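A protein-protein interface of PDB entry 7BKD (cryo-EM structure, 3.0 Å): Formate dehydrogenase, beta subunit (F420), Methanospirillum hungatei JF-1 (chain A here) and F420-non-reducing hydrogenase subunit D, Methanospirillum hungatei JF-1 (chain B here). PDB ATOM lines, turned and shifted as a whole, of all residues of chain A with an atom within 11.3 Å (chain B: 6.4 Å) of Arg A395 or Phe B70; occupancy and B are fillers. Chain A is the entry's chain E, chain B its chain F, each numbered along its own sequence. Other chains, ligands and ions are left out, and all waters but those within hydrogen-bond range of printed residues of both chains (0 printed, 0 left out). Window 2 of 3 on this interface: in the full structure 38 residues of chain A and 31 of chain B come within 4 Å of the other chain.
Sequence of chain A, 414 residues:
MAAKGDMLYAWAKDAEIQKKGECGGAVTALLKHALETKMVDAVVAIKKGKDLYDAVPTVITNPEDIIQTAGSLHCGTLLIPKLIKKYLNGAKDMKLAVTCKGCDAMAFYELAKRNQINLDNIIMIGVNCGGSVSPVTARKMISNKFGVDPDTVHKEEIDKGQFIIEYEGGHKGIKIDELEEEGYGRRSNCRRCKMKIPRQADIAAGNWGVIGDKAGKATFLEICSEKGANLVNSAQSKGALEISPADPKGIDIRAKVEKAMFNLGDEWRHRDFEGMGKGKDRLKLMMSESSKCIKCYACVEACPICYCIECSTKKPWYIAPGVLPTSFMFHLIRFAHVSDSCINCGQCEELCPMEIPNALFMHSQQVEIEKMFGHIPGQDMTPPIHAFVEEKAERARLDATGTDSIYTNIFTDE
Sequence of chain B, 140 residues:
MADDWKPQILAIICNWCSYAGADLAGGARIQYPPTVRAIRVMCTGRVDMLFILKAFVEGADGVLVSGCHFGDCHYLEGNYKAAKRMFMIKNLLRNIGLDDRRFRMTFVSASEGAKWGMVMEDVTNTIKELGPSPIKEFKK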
ATOM      1  N   PHE A 373       0.984  12.964  -2.699  1.00  0.00           N
ATOM      2  CA  PHE A 373       1.581  12.109  -3.718  1.00  0.00           C
ATOM      3  C   PHE A 373       0.623  11.060  -4.263  1.00  0.00           C
ATOM      4  O   PHE A 373       0.855  10.548  -5.361  1.00  0.00           O
ATOM      5  CB  PHE A 373       2.818  11.407  -3.167  1.00  0.00           C
ATOM      6  CG  PHE A 373       3.986  12.314  -2.952  1.00  0.00           C
ATOM      7  CD1 PHE A 373       4.718  12.782  -4.021  1.00  0.00           C
ATOM      8  CD2 PHE A 373       4.367  12.678  -1.679  1.00  0.00           C
ATOM      9  CE1 PHE A 373       5.795  13.609  -3.826  1.00  0.00           C
ATOM     10  CE2 PHE A 373       5.448  13.500  -1.478  1.00  0.00           C
ATOM     11  CZ  PHE A 373       6.163  13.967  -2.555  1.00  0.00           C
ATOM     12  N   VAL A 389      11.111   7.656  -9.565  1.00  0.00           N
ATOM     13  CA  VAL A 389      10.734   9.024  -9.891  1.00  0.00           C
ATOM     14  C   VAL A 389      10.538   9.115 -11.395  1.00  0.00           C
ATOM     15  O   VAL A 389      11.429   8.743 -12.166  1.00  0.00           O
ATOM     16  CB  VAL A 389      11.794  10.027  -9.413  1.00  0.00           C
ATOM     17  CG1 VAL A 389      11.478  11.407  -9.928  1.00  0.00           C
ATOM     18  CG2 VAL A 389      11.873  10.025  -7.902  1.00  0.00           C
ATOM     19  N   GLU A 390       9.379   9.611 -11.809  1.00  0.00           N
ATOM     20  CA  GLU A 390       9.029   9.736 -13.212  1.00  0.00           C
ATOM     21  C   GLU A 390       9.130  11.194 -13.649  1.00  0.00           C
ATOM     22  O   GLU A 390       8.890  12.113 -12.864  1.00  0.00           O
ATOM     23  CB  GLU A 390       7.619   9.197 -13.466  1.00  0.00           C
ATOM     24  CG  GLU A 390       7.320   8.873 -14.921  1.00  0.00           C
ATOM     25  CD  GLU A 390       6.630  10.010 -15.643  1.00  0.00           C
ATOM     26  OE1 GLU A 390       5.839  10.728 -14.999  1.00  0.00           O
ATOM     27  OE2 GLU A 390       6.881  10.190 -16.852  1.00  0.00           O
ATOM     28  N   GLU A 391       9.494  11.390 -14.916  1.00  0.00           N
ATOM     29  CA  GLU A 391       9.722  12.730 -15.448  1.00  0.00           C
ATOM     30  C   GLU A 391       8.435  13.549 -15.475  1.00  0.00           C
ATOM     31  O   GLU A 391       8.359  14.645 -14.900  1.00  0.00           O
ATOM     32  CB  GLU A 391      10.309  12.613 -16.855  1.00  0.00           C
ATOM     33  CG  GLU A 391      10.484  13.923 -17.584  1.00  0.00           C
ATOM     34  CD  GLU A 391      11.625  14.728 -17.025  1.00  0.00           C
ATOM     35  OE1 GLU A 391      12.481  14.132 -16.344  1.00  0.00           O
ATOM     36  OE2 GLU A 391      11.675  15.948 -17.279  1.00  0.00           O
ATOM     37  N   LYS A 392       7.411  13.028 -16.155  1.00  0.00           N
ATOM     38  CA  LYS A 392       6.167  13.770 -16.319  1.00  0.00           C
ATOM     39  C   LYS A 392       5.514  14.070 -14.982  1.00  0.00           C
ATOM     40  O   LYS A 392       4.907  15.133 -14.817  1.00  0.00           O
ATOM     41  CB  LYS A 392       5.202  12.991 -17.212  1.00  0.00           C
ATOM     42  CG  LYS A 392       5.390  13.235 -18.697  1.00  0.00           C
ATOM     43  CD  LYS A 392       6.488  12.358 -19.267  1.00  0.00           C
ATOM     44  CE  LYS A 392       6.859  12.787 -20.675  1.00  0.00           C
ATOM     45  NZ  LYS A 392       8.114  12.132 -21.139  1.00  0.00           N
ATOM     46  N   ALA A 393       5.625  13.155 -14.020  1.00  0.00           N
ATOM     47  CA  ALA A 393       5.024  13.381 -12.712  1.00  0.00           C
ATOM     48  C   ALA A 393       5.632  14.598 -12.033  1.00  0.00           C
ATOM     49  O   ALA A 393       4.913  15.448 -11.498  1.00  0.00           O
ATOM     50  CB  ALA A 393       5.190  12.137 -11.842  1.00  0.00           C
ATOM     51  N   GLU A 394       6.961  14.713 -12.062  1.00  0.00           N
ATOM     52  CA  GLU A 394       7.612  15.856 -11.432  1.00  0.00           C
ATOM     53  C   GLU A 394       7.324  17.144 -12.184  1.00  0.00           C
ATOM     54  O   GLU A 394       7.104  18.193 -11.565  1.00  0.00           O
ATOM     55  CB  GLU A 394       9.116  15.625 -11.335  1.00  0.00           C
ATOM     56  CG  GLU A 394       9.470  14.310 -10.698  1.00  0.00           C
ATOM     57  CD  GLU A 394       8.648  14.041  -9.458  1.00  0.00           C
ATOM     58  OE1 GLU A 394       8.527  14.955  -8.614  1.00  0.00           O
ATOM     59  OE2 GLU A 394       8.115  12.918  -9.328  1.00  0.00           O
ATOM     60  N   ARG A 395       7.324  17.092 -13.516  1.00  0.00           N
ATOM     61  CA  ARG A 395       7.019  18.303 -14.267  1.00  0.00           C
ATOM     62  C   ARG A 395       5.602  18.782 -13.979  1.00  0.00           C
ATOM     63  O   ARG A 395       5.377  19.980 -13.765  1.00  0.00           O
ATOM     64  CB  ARG A 395       7.230  18.066 -15.759  1.00  0.00           C
ATOM     65  CG  ARG A 395       8.647  18.367 -16.197  1.00  0.00           C
ATOM     66  CD  ARG A 395       8.803  18.328 -17.699  1.00  0.00           C
ATOM     67  NE  ARG A 395       9.838  19.257 -18.140  1.00  0.00           N
ATOM     68  CZ  ARG A 395      10.994  18.887 -18.676  1.00  0.00           C
ATOM     69  NH1 ARG A 395      11.267  17.602 -18.843  1.00  0.00           N
ATOM     70  NH2 ARG A 395      11.876  19.802 -19.048  1.00  0.00           N
ATOM     71  N   ALA A 396       4.638  17.861 -13.937  1.00  0.00           N
ATOM     72  CA  ALA A 396       3.264  18.237 -13.625  1.00  0.00           C
ATOM     73  C   ALA A 396       3.135  18.749 -12.197  1.00  0.00           C
ATOM     74  O   ALA A 396       2.385  19.697 -11.942  1.00  0.00           O
ATOM     75  CB  ALA A 396       2.331  17.049 -13.854  1.00  0.00           C
ATOM     76  N   ARG A 397       3.845  18.133 -11.250  1.00  0.00           N
ATOM     77  CA  ARG A 397       3.770  18.591  -9.867  1.00  0.00           C
ATOM     78  C   ARG A 397       4.332  19.996  -9.722  1.00  0.00           C
ATOM     79  O   ARG A 397       3.816  20.800  -8.939  1.00  0.00           O
ATOM     80  CB  ARG A 397       4.502  17.621  -8.944  1.00  0.00           C
ATOM     81  CG  ARG A 397       3.972  17.618  -7.523  1.00  0.00           C
ATOM     82  CD  ARG A 397       4.671  16.587  -6.660  1.00  0.00           C
ATOM     83  NE  ARG A 397       4.016  15.284  -6.724  1.00  0.00           N
ATOM     84  CZ  ARG A 397       4.542  14.212  -7.305  1.00  0.00           C
ATOM     85  NH1 ARG A 397       5.738  14.284  -7.872  1.00  0.00           N
ATOM     86  NH2 ARG A 397       3.875  13.067  -7.319  1.00  0.00           N
ATOM     87  N   LEU A 398       5.398  20.311 -10.457  1.00  0.00           N
ATOM     88  CA  LEU A 398       5.927  21.669 -10.407  1.00  0.00           C
ATOM     89  C   LEU A 398       4.988  22.653 -11.092  1.00  0.00           C
ATOM     90  O   LEU A 398       4.805  23.777 -10.614  1.00  0.00           O
ATOM     91  CB  LEU A 398       7.316  21.730 -11.038  1.00  0.00           C
ATOM     92  CG  LEU A 398       8.087  23.015 -10.729  1.00  0.00           C
ATOM     93  CD1 LEU A 398       7.886  23.427  -9.283  1.00  0.00           C
ATOM     94  CD2 LEU A 398       9.561  22.851 -11.036  1.00  0.00           C
ATOM     95  N   ASP A 399       4.388  22.250 -12.213  1.00  0.00           N
ATOM     96  CA  ASP A 399       3.509  23.154 -12.944  1.00  0.00           C
ATOM     97  C   ASP A 399       2.207  23.408 -12.198  1.00  0.00           C
ATOM     98  O   ASP A 399       1.583  24.458 -12.387  1.00  0.00           O
ATOM     99  CB  ASP A 399       3.217  22.589 -14.333  1.00  0.00           C
ATOM    100  CG  ASP A 399       4.458  22.495 -15.194  1.00  0.00           C
ATOM    101  OD1 ASP A 399       5.568  22.726 -14.668  1.00  0.00           O
ATOM    102  OD2 ASP A 399       4.326  22.190 -16.398  1.00  0.00           O
ATOM    103  N   ALA A 400       1.776  22.464 -11.359  1.00  0.00           N
ATOM    104  CA  ALA A 400       0.520  22.636 -10.639  1.00  0.00           C
ATOM    105  C   ALA A 400       0.569  23.817  -9.683  1.00  0.00           C
ATOM    106  O   ALA A 400      -0.471  24.414  -9.383  1.00  0.00           O
ATOM    107  CB  ALA A 400       0.169  21.357  -9.882  1.00  0.00           C
ATOM    108  N   THR A 401       1.753  24.169  -9.189  1.00  0.00           N
ATOM    109  CA  THR A 401       1.872  25.302  -8.284  1.00  0.00           C
ATOM    110  C   THR A 401       1.953  26.637  -9.008  1.00  0.00           C
ATOM    111  O   THR A 401       1.833  27.680  -8.358  1.00  0.00           O
ATOM    112  CB  THR A 401       3.098  25.141  -7.386  1.00  0.00           C
ATOM    113  OG1 THR A 401       4.287  25.300  -8.167  1.00  0.00           O
ATOM    114  CG2 THR A 401       3.101  23.768  -6.741  1.00  0.00           C
ATOM    115  N   GLY A 402       2.144  26.633 -10.323  1.00  0.00           N
ATOM    116  CA  GLY A 402       2.234  27.880 -11.064  1.00  0.00           C
ATOM    117  C   GLY A 402       3.362  28.775 -10.606  1.00  0.00           C
ATOM    118  O   GLY A 402       3.183  29.994 -10.498  1.00  0.00           O
ATOM    119  N   THR A 403       4.525  28.195 -10.324  1.00  0.00           N
ATOM    120  CA  THR A 403       5.660  28.957  -9.829  1.00  0.00           C
ATOM    121  C   THR A 403       6.935  28.285 -10.319  1.00  0.00           C
ATOM    122  O   THR A 403       6.976  27.073 -10.537  1.00  0.00           O
ATOM    123  CB  THR A 403       5.631  29.060  -8.294  1.00  0.00           C
ATOM    124  OG1 THR A 403       4.399  29.666  -7.882  1.00  0.00           O
ATOM    125  CG2 THR A 403       6.780  29.908  -7.770  1.00  0.00           C
ATOM    126  N   ASP A 404       7.976  29.091 -10.498  1.00  0.00           N
ATOM    127  CA  ASP A 404       9.251  28.615 -11.013  1.00  0.00           C
ATOM    128  C   ASP A 404      10.112  27.942  -9.953  1.00  0.00           C
ATOM    129  O   ASP A 404      11.229  27.518 -10.265  1.00  0.00           O
ATOM    130  CB  ASP A 404      10.024  29.777 -11.634  1.00  0.00           C
ATOM    131  CG  ASP A 404      10.121  30.971 -10.704  1.00  0.00           C
ATOM    132  OD1 ASP A 404       9.493  30.937  -9.624  1.00  0.00           O
ATOM    133  OD2 ASP A 404      10.826  31.941 -11.050  1.00  0.00           O
ATOM    134  N   SER A 405       9.635  27.836  -8.715  1.00  0.00           N
ATOM    135  CA  SER A 405      10.425  27.250  -7.647  1.00  0.00           C
ATOM    136  C   SER A 405       9.507  26.523  -6.679  1.00  0.00           C
ATOM    137  O   SER A 405       8.287  26.697  -6.701  1.00  0.00           O
ATOM    138  CB  SER A 405      11.241  28.309  -6.904  1.00  0.00           C
ATOM    139  OG  SER A 405      10.448  28.965  -5.933  1.00  0.00           O
ATOM    140  N   ILE A 406      10.110  25.689  -5.839  1.00  0.00           N
ATOM    141  CA  ILE A 406       9.363  24.966  -4.798  1.00  0.00           C
ATOM    142  C   ILE A 406       9.409  25.856  -3.563  1.00  0.00           C
ATOM    143  O   ILE A 406      10.212  25.677  -2.648  1.00  0.00           O
ATOM    144  CB  ILE A 406       9.940  23.572  -4.547  1.00  0.00           C
ATOM    145  CG1 ILE A 406       9.824  22.717  -5.805  1.00  0.00           C
ATOM    146  CG2 ILE A 406       9.217  22.886  -3.405  1.00  0.00           C
ATOM    147  CD1 ILE A 406      10.592  21.432  -5.732  1.00  0.00           C
ATOM    148  N   TYR A 407       8.539  26.860  -3.546  1.00  0.00           N
ATOM    149  CA  TYR A 407       8.474  27.771  -2.410  1.00  0.00           C
ATOM    150  C   TYR A 407       7.104  27.812  -1.754  1.00  0.00           C
ATOM    151  O   TYR A 407       6.998  27.570  -0.547  1.00  0.00           O
ATOM    152  CB  TYR A 407       8.898  29.179  -2.846  1.00  0.00           C
ATOM    153  CG  TYR A 407       8.747  30.221  -1.768  1.00  0.00           C
ATOM    154  CD1 TYR A 407       9.196  29.982  -0.482  1.00  0.00           C
ATOM    155  CD2 TYR A 407       8.173  31.448  -2.043  1.00  0.00           C
ATOM    156  CE1 TYR A 407       9.061  30.929   0.505  1.00  0.00           C
ATOM    157  CE2 TYR A 407       8.035  32.401  -1.062  1.00  0.00           C
ATOM    158  CZ  TYR A 407       8.480  32.138   0.209  1.00  0.00           C
ATOM    159  OH  TYR A 407       8.345  33.090   1.190  1.00  0.00           O
ATOM    160  N   CYS B  68      19.422  22.831 -11.229  1.00  0.00           N
ATOM    161  CA  CYS B  68      19.307  23.158 -12.637  1.00  0.00           C
ATOM    162  C   CYS B  68      17.848  23.087 -13.061  1.00  0.00           C
ATOM    163  O   CYS B  68      17.049  22.361 -12.469  1.00  0.00           O
ATOM    164  CB  CYS B  68      20.139  22.199 -13.491  1.00  0.00           C
ATOM    165  SG  CYS B  68      21.753  21.764 -12.809  1.00  0.00           S
ATOM    166  N   HIS B  69      17.507  23.847 -14.096  1.00  0.00           N
ATOM    167  CA  HIS B  69      16.158  23.792 -14.637  1.00  0.00           C
ATOM    168  C   HIS B  69      15.856  22.385 -15.131  1.00  0.00           C
ATOM    169  O   HIS B  69      16.747  21.651 -15.561  1.00  0.00           O
ATOM    170  CB  HIS B  69      15.998  24.790 -15.782  1.00  0.00           C
ATOM    171  CG  HIS B  69      15.848  26.208 -15.333  1.00  0.00           C
ATOM    172  ND1 HIS B  69      16.849  27.143 -15.479  1.00  0.00           N
ATOM    173  CD2 HIS B  69      14.812  26.853 -14.747  1.00  0.00           C
ATOM    174  CE1 HIS B  69      16.438  28.302 -14.998  1.00  0.00           C
ATOM    175  NE2 HIS B  69      15.205  28.153 -14.549  1.00  0.00           N
ATOM    176  N   PHE B  70      14.586  22.002 -15.050  1.00  0.00           N
ATOM    177  CA  PHE B  70      14.189  20.669 -15.475  1.00  0.00           C
ATOM    178  C   PHE B  70      14.547  20.455 -16.939  1.00  0.00           C
ATOM    179  O   PHE B  70      14.242  21.290 -17.794  1.00  0.00           O
ATOM    180  CB  PHE B  70      12.692  20.470 -15.259  1.00  0.00           C
ATOM    181  CG  PHE B  70      12.324  20.151 -13.842  1.00  0.00           C
ATOM    182  CD1 PHE B  70      13.298  20.025 -12.871  1.00  0.00           C
ATOM    183  CD2 PHE B  70      11.004  19.972 -13.481  1.00  0.00           C
ATOM    184  CE1 PHE B  70      12.963  19.733 -11.571  1.00  0.00           C
ATOM    185  CE2 PHE B  70      10.668  19.679 -12.183  1.00  0.00           C
ATOM    186  CZ  PHE B  70      11.648  19.559 -11.227  1.00  0.00           C
ATOM    187  N   GLY B  71      15.193  19.329 -17.223  1.00  0.00           N
ATOM    188  CA  GLY B  71      15.726  19.061 -18.538  1.00  0.00           C
ATOM    189  C   GLY B  71      17.103  19.627 -18.794  1.00  0.00           C
ATOM    190  O   GLY B  71      17.630  19.450 -19.898  1.00  0.00           O
ATOM    191  N   ASP B  72      17.707  20.296 -17.813  1.00  0.00           N
ATOM    192  CA  ASP B  72      19.023  20.897 -17.976  1.00  0.00           C
ATOM    193  C   ASP B  72      20.045  20.356 -16.989  1.00  0.00           C
ATOM    194  O   ASP B  72      21.124  20.941 -16.852  1.00  0.00           O
ATOM    195  CB  ASP B  72      18.936  22.417 -17.836  1.00  0.00           C
ATOM    196  CG  ASP B  72      18.161  23.062 -18.963  1.00  0.00           C
ATOM    197  OD1 ASP B  72      17.728  24.221 -18.801  1.00  0.00           O
ATOM    198  OD2 ASP B  72      17.984  22.407 -20.012  1.00  0.00           O
ATOM    199  N   CYS B  73      19.740  19.263 -16.295  1.00  0.00           N
ATOM    200  CA  CYS B  73      20.687  18.693 -15.349  1.00  0.00           C
ATOM    201  C   CYS B  73      21.894  18.130 -16.083  1.00  0.00           C
ATOM    202  O   CYS B  73      21.768  17.544 -17.160  1.00  0.00           O
ATOM    203  CB  CYS B  73      20.020  17.594 -14.523  1.00  0.00           C
ATOM    204  SG  CYS B  73      21.011  16.987 -13.145  1.00  0.00           S
ATOM    205  N   ASN B  79      17.842  16.509 -10.729  1.00  0.00           N
ATOM    206  CA  ASN B  79      16.985  17.525 -10.145  1.00  0.00           C
ATOM    207  C   ASN B  79      15.556  17.041  -9.954  1.00  0.00           C
ATOM    208  O   ASN B  79      14.847  17.592  -9.115  1.00  0.00           O
ATOM    209  CB  ASN B  79      17.029  18.796 -10.992  1.00  0.00           C
ATOM    210  CG  ASN B  79      16.787  18.531 -12.454  1.00  0.00           C
ATOM    211  OD1 ASN B  79      16.503  17.408 -12.857  1.00  0.00           O
ATOM    212  ND2 ASN B  79      16.906  19.569 -13.265  1.00  0.00           N
ATOM    213  N   TYR B  80      15.127  16.000 -10.665  1.00  0.00           N
ATOM    214  CA  TYR B  80      13.800  15.449 -10.410  1.00  0.00           C
ATOM    215  C   TYR B  80      13.761  14.681  -9.096  1.00  0.00           C
ATOM    216  O   TYR B  80      12.801  14.805  -8.322  1.00  0.00           O
ATOM    217  CB  TYR B  80      13.378  14.560 -11.573  1.00  0.00           C
ATOM    218  CG  TYR B  80      13.551  15.239 -12.899  1.00  0.00           C
ATOM    219  CD1 TYR B  80      12.703  16.260 -13.289  1.00  0.00           C
ATOM    220  CD2 TYR B  80      14.572  14.876 -13.753  1.00  0.00           C
ATOM    221  CE1 TYR B  80      12.861  16.891 -14.496  1.00  0.00           C
ATOM    222  CE2 TYR B  80      14.740  15.505 -14.962  1.00  0.00           C
ATOM    223  CZ  TYR B  80      13.883  16.511 -15.328  1.00  0.00           C
ATOM    224  OH  TYR B  80      14.046  17.136 -16.539  1.00  0.00           O
ATOM    225  N   ALA B  83      13.706  17.258  -6.553  1.00  0.00           N
ATOM    226  CA  ALA B  83      12.398  17.889  -6.431  1.00  0.00           C
ATOM    227  C   ALA B  83      11.442  17.034  -5.613  1.00  0.00           C
ATOM    228  O   ALA B  83      10.711  17.557  -4.764  1.00  0.00           O
ATOM    229  CB  ALA B  83      11.821  18.164  -7.817  1.00  0.00           C
ATOM    230  N   MET B 105      13.592  25.474  -2.700  1.00  0.00           N
ATOM    231  CA  MET B 105      14.471  24.998  -3.756  1.00  0.00           C
ATOM    232  C   MET B 105      14.226  25.812  -5.016  1.00  0.00           C
ATOM    233  O   MET B 105      13.102  25.863  -5.522  1.00  0.00           O
ATOM    234  CB  MET B 105      14.258  23.513  -4.046  1.00  0.00           C
ATOM    235  CG  MET B 105      15.267  22.957  -5.032  1.00  0.00           C
ATOM    236  SD  MET B 105      15.063  21.226  -5.452  1.00  0.00           S
ATOM    237  CE  MET B 105      15.943  21.166  -7.003  1.00  0.00           C
ATOM    238  N   PHE B 107      15.637  27.031  -9.076  1.00  0.00           N
ATOM    239  CA  PHE B 107      16.217  26.497 -10.303  1.00  0.00           C
ATOM    240  C   PHE B 107      16.934  27.638 -11.012  1.00  0.00           C
ATOM    241  O   PHE B 107      16.319  28.398 -11.765  1.00  0.00           O
ATOM    242  CB  PHE B 107      15.144  25.871 -11.181  1.00  0.00           C
ATOM    243  CG  PHE B 107      14.419  24.737 -10.525  1.00  0.00           C
ATOM    244  CD1 PHE B 107      14.973  23.474 -10.492  1.00  0.00           C
ATOM    245  CD2 PHE B 107      13.191  24.935  -9.930  1.00  0.00           C
ATOM    246  CE1 PHE B 107      14.313  22.433  -9.888  1.00  0.00           C
ATOM    247  CE2 PHE B 107      12.529  23.895  -9.321  1.00  0.00           C
ATOM    248  CZ  PHE B 107      13.090  22.644  -9.301  1.00  0.00           C
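Of the printed residues of chain B, Glu A394 touches Phe B70. Arg A395 touches just these residues of chain B: Phe B70 (3.1 Å), Gly B71 (3.8 Å) and Tyr B80 (3.6 Å). Of the printed residues of chain B, Asp A404 touches Phe B107 (3.3 Å). No residue of chain A comes within 4 Å of His B69. Phe B70 touches just these residues of chain A: Glu A394, Arg A395 and Leu A398. No residue of chain A comes within 4 Å of Asn B79. Printed residues of chain A within 4 Å of Met B105: Ser A405 (3.4 Å) and Ile A406 (3.0 Å). Of the printed residues of chain A, Phe B107 touches Leu A398 (3.6 Å) and Asp A404 (3.3 Å).
O of Phe B70 sits at hydrogen-bond distance from NH2 of Arg A395, at 3.1 Å. The side-chain hydroxyl (OH) of Tyr B80 is in hydrogen-bond range of the side-chain carboxylate (OE2) of Glu A391 (2.8 Å). O of Met B105 sits at hydrogen-bond distance from N of Ile A406, at 3.0 Å.
Among the printed residues, pairs that only touch across the chains: Asp A404 with Phe B107 (3.3 Å), Ser A405 with Met B105 (3.4 Å), Leu A398 with Phe B70 (3.6 Å), Leu A398 with Phe B107 (3.6 Å), Arg A395 with Tyr B80 (3.6 Å), Arg A395 with Gly B71 (3.8 Å), Glu A394 with Phe B70 (3.9 Å), Val A389 with Tyr B80 (3.98 Å) and Ile A406 with Ala B83 (3.996 Å).
The backbone carbonyl oxygen (O) of Phe B107 sits at hydrogen-bond distance from a ring nitrogen (NE2) of His B69. The side-chain hydroxyl (OH) of Tyr B80 lies within hydrogen-bond range of the backbone NH (N) of Gly B71, 2.6 Å away. NE of Arg A395 is in salt-bridge range of OE2 of Glu A391 (3.9 Å). The side-chain carboxylate (OE1) of Glu A394 lies within salt-bridge range of the guanidinium group (NH1) of Arg A397 (3.0 Å). O of Leu A398 is in hydrogen-bond range of OG1 of Thr A401.
Printed residues of chain B that touch a printed residue of chain A: Phe B70, Gly B71, Tyr B80, Ala B83, Met B105 and Phe B107. Hydrophobic or aromatic side chains of chain B that line the printed part of chain A: Phe B70, Tyr B80 and Phe B107. Among the printed residues, 12 pairs touch across the chains.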
